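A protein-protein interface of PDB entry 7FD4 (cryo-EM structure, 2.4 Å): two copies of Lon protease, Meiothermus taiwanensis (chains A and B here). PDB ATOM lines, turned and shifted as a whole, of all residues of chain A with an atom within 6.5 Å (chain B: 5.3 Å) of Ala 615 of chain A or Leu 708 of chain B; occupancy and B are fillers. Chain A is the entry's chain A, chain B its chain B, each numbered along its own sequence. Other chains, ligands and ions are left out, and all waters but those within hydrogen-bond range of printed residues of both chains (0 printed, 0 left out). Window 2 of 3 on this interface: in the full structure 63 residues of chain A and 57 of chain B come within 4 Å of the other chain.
Of the 8 printed residues of chain B, 5 touch a printed residue of chain A.
Along chain A the printed residues that touch a printed residue of chain B span positions 613 to 666.
Among the printed residues, merely in contact across the chains: Glu 613 of chain A with Ser 707 of chain B, His 664 of chain A with Leu 708 of chain B, His 666 of chain A with Leu 708 of chain B, His 664 of chain A with Ala 639 of chain B, Val 614 of chain A with Leu 708 of chain B and Ala 615 of chain A with Leu 708 of chain B.
The backbone carbonyl oxygen of Gly 595 of chain A sits at hydrogen-bond distance from the backbone NH of Val 614 of chain A, 3.0 Å away.
N of His 666 of chain A sits at hydrogen-bond distance from O of Glu 613 of chain A (3.0 Å).
N of Ala 615 of chain A sits at hydrogen-bond distance from O of His 664 of chain A, 3.2 Å away.
The side-chain hydroxyl of Thr 626 of chain A lies within hydrogen-bond range of a ring nitrogen (NE2) of His 664 of chain A, at 2.7 Å.
OG1 of Thr 626 of chain A is in hydrogen-bond range of ND1 of His 666 of chain A (3.2 Å).
ND1 of His 664 of chain A lies within hydrogen-bond range of OG1 of Thr 642 of chain B.
The side-chain carboxylate (OE2) of Glu 613 of chain A lies within hydrogen-bond range of the backbone NH (N) of Leu 708 of chain B (3.2 Å).
The guanidinium group of Arg 709 of chain B lies within salt-bridge range of the side-chain carboxylate of Glu 613 of chain A (2.8 Å).
No position is printed for both chains.
Of the printed residues of chain A, Leu 708 of chain B touches Glu 613 (3.2 Å), Val 614 (3.98 Å), Ala 615 (3.99 Å), His 664 (3.6 Å) and His 666 (3.8 Å).
Printed residues of chain B within 4 Å of Glu 613 of chain A: Ser 707 (3.3 Å), Leu 708 (3.2 Å) and Arg 709 (2.8 Å).
Of the printed residues of chain A, Arg 709 of chain B touches Glu 613 (2.8 Å).
Asp 662 of chain A touches none of the printed residues of chain B.
Thr 626 of chain A touches none of the printed residues of chain B.
The nearest printed residue of chain B that does not touch Ala 615 of chain A is Thr 642 of chain B (4.3 Å).
The nearest printed residue of chain A that does not touch Leu 708 of chain B is Val 665 of chain A (4.9 Å).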
ATOM      1  N   GLY A 595     -15.359 -11.036 -10.475  1.00  0.00           N
ATOM      2  CA  GLY A 595     -15.444 -12.442 -10.151  1.00  0.00           C
ATOM      3  C   GLY A 595     -16.768 -13.069 -10.499  1.00  0.00           C
ATOM      4  O   GLY A 595     -17.299 -13.855  -9.715  1.00  0.00           O
ATOM      5  N   GLU A 613     -20.093 -17.509 -10.100  1.00  0.00           N
ATOM      6  CA  GLU A 613     -19.490 -16.492  -9.262  1.00  0.00           C
ATOM      7  C   GLU A 613     -18.473 -17.126  -8.333  1.00  0.00           C
ATOM      8  O   GLU A 613     -18.645 -18.253  -7.874  1.00  0.00           O
ATOM      9  CB  GLU A 613     -20.555 -15.739  -8.500  1.00  0.00           C
ATOM     10  CG  GLU A 613     -21.426 -16.608  -7.667  1.00  0.00           C
ATOM     11  CD  GLU A 613     -22.636 -15.877  -7.173  1.00  0.00           C
ATOM     12  OE1 GLU A 613     -22.802 -14.697  -7.530  1.00  0.00           O
ATOM     13  OE2 GLU A 613     -23.429 -16.481  -6.432  1.00  0.00           O
ATOM     14  N   VAL A 614     -17.365 -16.423  -8.130  1.00  0.00           N
ATOM     15  CA  VAL A 614     -16.266 -16.903  -7.306  1.00  0.00           C
ATOM     16  C   VAL A 614     -15.827 -15.791  -6.369  1.00  0.00           C
ATOM     17  O   VAL A 614     -16.139 -14.616  -6.575  1.00  0.00           O
ATOM     18  CB  VAL A 614     -15.056 -17.375  -8.135  1.00  0.00           C
ATOM     19  CG1 VAL A 614     -15.406 -18.501  -9.041  1.00  0.00           C
ATOM     20  CG2 VAL A 614     -14.607 -16.296  -8.954  1.00  0.00           C
ATOM     21  N   ALA A 615     -15.091 -16.167  -5.335  1.00  0.00           N
ATOM     22  CA  ALA A 615     -14.580 -15.223  -4.357  1.00  0.00           C
ATOM     23  C   ALA A 615     -13.191 -15.644  -3.924  1.00  0.00           C
ATOM     24  O   ALA A 615     -12.939 -16.824  -3.697  1.00  0.00           O
ATOM     25  CB  ALA A 615     -15.476 -15.144  -3.141  1.00  0.00           C
ATOM     26  N   ALA A 616     -12.295 -14.680  -3.799  1.00  0.00           N
ATOM     27  CA  ALA A 616     -10.936 -14.936  -3.348  1.00  0.00           C
ATOM     28  C   ALA A 616     -10.764 -14.284  -1.990  1.00  0.00           C
ATOM     29  O   ALA A 616     -10.816 -13.058  -1.877  1.00  0.00           O
ATOM     30  CB  ALA A 616      -9.916 -14.404  -4.343  1.00  0.00           C
ATOM     31  N   VAL A 617     -10.567 -15.096  -0.966  1.00  0.00           N
ATOM     32  CA  VAL A 617     -10.415 -14.611   0.401  1.00  0.00           C
ATOM     33  C   VAL A 617      -9.033 -15.035   0.865  1.00  0.00           C
ATOM     34  O   VAL A 617      -8.455 -15.982   0.310  1.00  0.00           O
ATOM     35  CB  VAL A 617     -11.536 -15.147   1.320  1.00  0.00           C
ATOM     36  CG1 VAL A 617     -12.859 -14.641   0.852  1.00  0.00           C
ATOM     37  CG2 VAL A 617     -11.536 -16.633   1.313  1.00  0.00           C
ATOM     38  N   THR A 626     -19.008 -25.516  -4.783  1.00  0.00           N
ATOM     39  CA  THR A 626     -20.333 -25.787  -4.256  1.00  0.00           C
ATOM     40  C   THR A 626     -21.406 -25.441  -5.274  1.00  0.00           C
ATOM     41  O   THR A 626     -21.159 -24.755  -6.262  1.00  0.00           O
ATOM     42  CB  THR A 626     -20.584 -25.022  -2.953  1.00  0.00           C
ATOM     43  OG1 THR A 626     -20.440 -23.617  -3.177  1.00  0.00           O
ATOM     44  CG2 THR A 626     -19.612 -25.459  -1.888  1.00  0.00           C
ATOM     45  N   VAL A 661      -4.098 -17.795  -0.772  1.00  0.00           N
ATOM     46  CA  VAL A 661      -5.437 -17.383  -1.161  1.00  0.00           C
ATOM     47  C   VAL A 661      -6.303 -18.623  -1.236  1.00  0.00           C
ATOM     48  O   VAL A 661      -5.886 -19.641  -1.789  1.00  0.00           O
ATOM     49  CB  VAL A 661      -5.414 -16.633  -2.506  1.00  0.00           C
ATOM     50  CG1 VAL A 661      -6.784 -16.412  -3.042  1.00  0.00           C
ATOM     51  CG2 VAL A 661      -4.767 -15.299  -2.335  1.00  0.00           C
ATOM     52  N   ASP A 662      -7.497 -18.544  -0.670  1.00  0.00           N
ATOM     53  CA  ASP A 662      -8.464 -19.626  -0.685  1.00  0.00           C
ATOM     54  C   ASP A 662      -9.598 -19.251  -1.631  1.00  0.00           C
ATOM     55  O   ASP A 662     -10.139 -18.150  -1.540  1.00  0.00           O
ATOM     56  CB  ASP A 662      -8.962 -19.858   0.736  1.00  0.00           C
ATOM     57  CG  ASP A 662      -9.673 -21.160   0.906  1.00  0.00           C
ATOM     58  OD1 ASP A 662      -9.958 -21.832  -0.100  1.00  0.00           O
ATOM     59  OD2 ASP A 662      -9.908 -21.544   2.068  1.00  0.00           O
ATOM     60  N   LEU A 663      -9.952 -20.156  -2.539  1.00  0.00           N
ATOM     61  CA  LEU A 663     -10.963 -19.899  -3.554  1.00  0.00           C
ATOM     62  C   LEU A 663     -12.235 -20.679  -3.273  1.00  0.00           C
ATOM     63  O   LEU A 663     -12.194 -21.771  -2.713  1.00  0.00           O
ATOM     64  CB  LEU A 663     -10.462 -20.269  -4.946  1.00  0.00           C
ATOM     65  CG  LEU A 663      -9.378 -19.397  -5.555  1.00  0.00           C
ATOM     66  CD1 LEU A 663      -8.904 -20.004  -6.829  1.00  0.00           C
ATOM     67  CD2 LEU A 663      -9.932 -18.046  -5.833  1.00  0.00           C
ATOM     68  N   HIS A 664     -13.362 -20.113  -3.681  1.00  0.00           N
ATOM     69  CA  HIS A 664     -14.661 -20.751  -3.565  1.00  0.00           C
ATOM     70  C   HIS A 664     -15.433 -20.460  -4.836  1.00  0.00           C
ATOM     71  O   HIS A 664     -15.564 -19.302  -5.220  1.00  0.00           O
ATOM     72  CB  HIS A 664     -15.417 -20.237  -2.344  1.00  0.00           C
ATOM     73  CG  HIS A 664     -16.711 -20.941  -2.075  1.00  0.00           C
ATOM     74  ND1 HIS A 664     -17.615 -20.487  -1.147  1.00  0.00           N
ATOM     75  CD2 HIS A 664     -17.258 -22.049  -2.614  1.00  0.00           C
ATOM     76  CE1 HIS A 664     -18.660 -21.289  -1.120  1.00  0.00           C
ATOM     77  NE2 HIS A 664     -18.471 -22.244  -2.006  1.00  0.00           N
ATOM     78  N   VAL A 665     -15.944 -21.501  -5.476  1.00  0.00           N
ATOM     79  CA  VAL A 665     -16.645 -21.398  -6.747  1.00  0.00           C
ATOM     80  C   VAL A 665     -18.064 -21.870  -6.502  1.00  0.00           C
ATOM     81  O   VAL A 665     -18.285 -23.055  -6.247  1.00  0.00           O
ATOM     82  CB  VAL A 665     -15.982 -22.248  -7.833  1.00  0.00           C
ATOM     83  CG1 VAL A 665     -16.718 -22.109  -9.131  1.00  0.00           C
ATOM     84  CG2 VAL A 665     -14.526 -21.906  -7.984  1.00  0.00           C
ATOM     85  N   HIS A 666     -19.022 -20.964  -6.578  1.00  0.00           N
ATOM     86  CA  HIS A 666     -20.417 -21.274  -6.307  1.00  0.00           C
ATOM     87  C   HIS A 666     -21.236 -21.029  -7.558  1.00  0.00           C
ATOM     88  O   HIS A 666     -21.122 -19.972  -8.174  1.00  0.00           O
ATOM     89  CB  HIS A 666     -20.934 -20.414  -5.160  1.00  0.00           C
ATOM     90  CG  HIS A 666     -22.374 -20.623  -4.839  1.00  0.00           C
ATOM     91  ND1 HIS A 666     -22.841 -21.755  -4.212  1.00  0.00           N
ATOM     92  CD2 HIS A 666     -23.447 -19.825  -5.021  1.00  0.00           C
ATOM     93  CE1 HIS A 666     -24.146 -21.657  -4.049  1.00  0.00           C
ATOM     94  NE2 HIS A 666     -24.537 -20.493  -4.530  1.00  0.00           N
ATOM     95  N   PRO A 668     -24.979 -20.720  -8.494  1.00  0.00           N
ATOM     96  CA  PRO A 668     -26.354 -20.668  -8.004  1.00  0.00           C
ATOM     97  C   PRO A 668     -27.328 -21.140  -9.066  1.00  0.00           C
ATOM     98  O   PRO A 668     -27.124 -20.910 -10.257  1.00  0.00           O
ATOM     99  CB  PRO A 668     -26.551 -19.184  -7.683  1.00  0.00           C
ATOM    100  CG  PRO A 668     -25.617 -18.498  -8.547  1.00  0.00           C
ATOM    101  CD  PRO A 668     -24.425 -19.375  -8.679  1.00  0.00           C
ATOM    102  N   ALA A 690     -11.511 -12.680 -10.291  1.00  0.00           N
ATOM    103  CA  ALA A 690     -11.436 -12.603  -8.841  1.00  0.00           C
ATOM    104  C   ALA A 690     -10.011 -12.423  -8.352  1.00  0.00           C
ATOM    105  O   ALA A 690      -9.778 -11.686  -7.394  1.00  0.00           O
ATOM    106  CB  ALA A 690     -12.033 -13.844  -8.211  1.00  0.00           C
ATOM    107  N   ALA B 639     -21.444 -21.086   1.887  1.00  0.00           N
ATOM    108  CA  ALA B 639     -21.577 -19.864   1.100  1.00  0.00           C
ATOM    109  C   ALA B 639     -21.750 -18.639   1.985  1.00  0.00           C
ATOM    110  O   ALA B 639     -21.141 -17.588   1.725  1.00  0.00           O
ATOM    111  CB  ALA B 639     -22.747 -19.993   0.136  1.00  0.00           C
ATOM    112  N   THR B 642     -18.369 -17.812   3.517  1.00  0.00           N
ATOM    113  CA  THR B 642     -17.427 -17.194   2.587  1.00  0.00           C
ATOM    114  C   THR B 642     -17.767 -15.732   2.339  1.00  0.00           C
ATOM    115  O   THR B 642     -16.861 -14.895   2.224  1.00  0.00           O
ATOM    116  CB  THR B 642     -17.405 -17.977   1.283  1.00  0.00           C
ATOM    117  OG1 THR B 642     -17.072 -19.335   1.567  1.00  0.00           O
ATOM    118  CG2 THR B 642     -16.363 -17.438   0.343  1.00  0.00           C
ATOM    119  N   TYR B 643     -19.063 -15.398   2.286  1.00  0.00           N
ATOM    120  CA  TYR B 643     -19.448 -13.988   2.211  1.00  0.00           C
ATOM    121  C   TYR B 643     -18.956 -13.207   3.420  1.00  0.00           C
ATOM    122  O   TYR B 643     -18.402 -12.106   3.279  1.00  0.00           O
ATOM    123  CB  TYR B 643     -20.960 -13.841   2.094  1.00  0.00           C
ATOM    124  CG  TYR B 643     -21.410 -12.399   2.121  1.00  0.00           C
ATOM    125  CD1 TYR B 643     -21.266 -11.596   1.012  1.00  0.00           C
ATOM    126  CD2 TYR B 643     -21.960 -11.839   3.263  1.00  0.00           C
ATOM    127  CE1 TYR B 643     -21.660 -10.289   1.033  1.00  0.00           C
ATOM    128  CE2 TYR B 643     -22.332 -10.533   3.296  1.00  0.00           C
ATOM    129  CZ  TYR B 643     -22.194  -9.765   2.175  1.00  0.00           C
ATOM    130  OH  TYR B 643     -22.586  -8.454   2.203  1.00  0.00           O
ATOM    131  N   VAL B 706     -29.167 -17.400   0.060  1.00  0.00           N
ATOM    132  CA  VAL B 706     -28.073 -16.460  -0.113  1.00  0.00           C
ATOM    133  C   VAL B 706     -27.170 -16.971  -1.226  1.00  0.00           C
ATOM    134  O   VAL B 706     -27.094 -18.175  -1.488  1.00  0.00           O
ATOM    135  CB  VAL B 706     -27.320 -16.263   1.223  1.00  0.00           C
ATOM    136  CG1 VAL B 706     -26.536 -17.485   1.606  1.00  0.00           C
ATOM    137  CG2 VAL B 706     -26.449 -15.035   1.205  1.00  0.00           C
ATOM    138  N   SER B 707     -26.546 -16.049  -1.939  1.00  0.00           N
ATOM    139  CA  SER B 707     -25.536 -16.382  -2.925  1.00  0.00           C
ATOM    140  C   SER B 707     -24.183 -15.918  -2.422  1.00  0.00           C
ATOM    141  O   SER B 707     -24.054 -15.381  -1.324  1.00  0.00           O
ATOM    142  CB  SER B 707     -25.850 -15.745  -4.272  1.00  0.00           C
ATOM    143  OG  SER B 707     -25.657 -14.352  -4.208  1.00  0.00           O
ATOM    144  N   LEU B 708     -23.167 -16.108  -3.248  1.00  0.00           N
ATOM    145  CA  LEU B 708     -21.815 -15.801  -2.820  1.00  0.00           C
ATOM    146  C   LEU B 708     -21.514 -14.315  -2.892  1.00  0.00           C
ATOM    147  O   LEU B 708     -20.595 -13.851  -2.219  1.00  0.00           O
ATOM    148  CB  LEU B 708     -20.827 -16.595  -3.665  1.00  0.00           C
ATOM    149  CG  LEU B 708     -19.404 -16.761  -3.176  1.00  0.00           C
ATOM    150  CD1 LEU B 708     -19.466 -17.511  -1.897  1.00  0.00           C
ATOM    151  CD2 LEU B 708     -18.647 -17.551  -4.181  1.00  0.00           C
ATOM    152  N   ARG B 709     -22.273 -13.557  -3.674  1.00  0.00           N
ATOM    153  CA  ARG B 709     -22.143 -12.110  -3.705  1.00  0.00           C
ATOM    154  C   ARG B 709     -23.019 -11.412  -2.687  1.00  0.00           C
ATOM    155  O   ARG B 709     -22.917 -10.192  -2.544  1.00  0.00           O
ATOM    156  CB  ARG B 709     -22.503 -11.564  -5.079  1.00  0.00           C
ATOM    157  CG  ARG B 709     -21.521 -11.865  -6.158  1.00  0.00           C
ATOM    158  CD  ARG B 709     -22.009 -11.281  -7.456  1.00  0.00           C
ATOM    159  NE  ARG B 709     -23.166 -12.001  -7.963  1.00  0.00           N
ATOM    160  CZ  ARG B 709     -23.865 -11.630  -9.025  1.00  0.00           C
ATOM    161  NH1 ARG B 709     -23.531 -10.537  -9.688  1.00  0.00           N
ATOM    162  NH2 ARG B 709     -24.899 -12.355  -9.420  1.00  0.00           N
ATOM    163  N   GLY B 710     -23.882 -12.140  -1.997  1.00  0.00           N
ATOM    164  CA  GLY B 710     -24.788 -11.546  -1.052  1.00  0.00           C
ATOM    165  C   GLY B 710     -26.171 -11.268  -1.573  1.00  0.00           C
ATOM    166  O   GLY B 710     -26.921 -10.552  -0.914  1.00  0.00           O
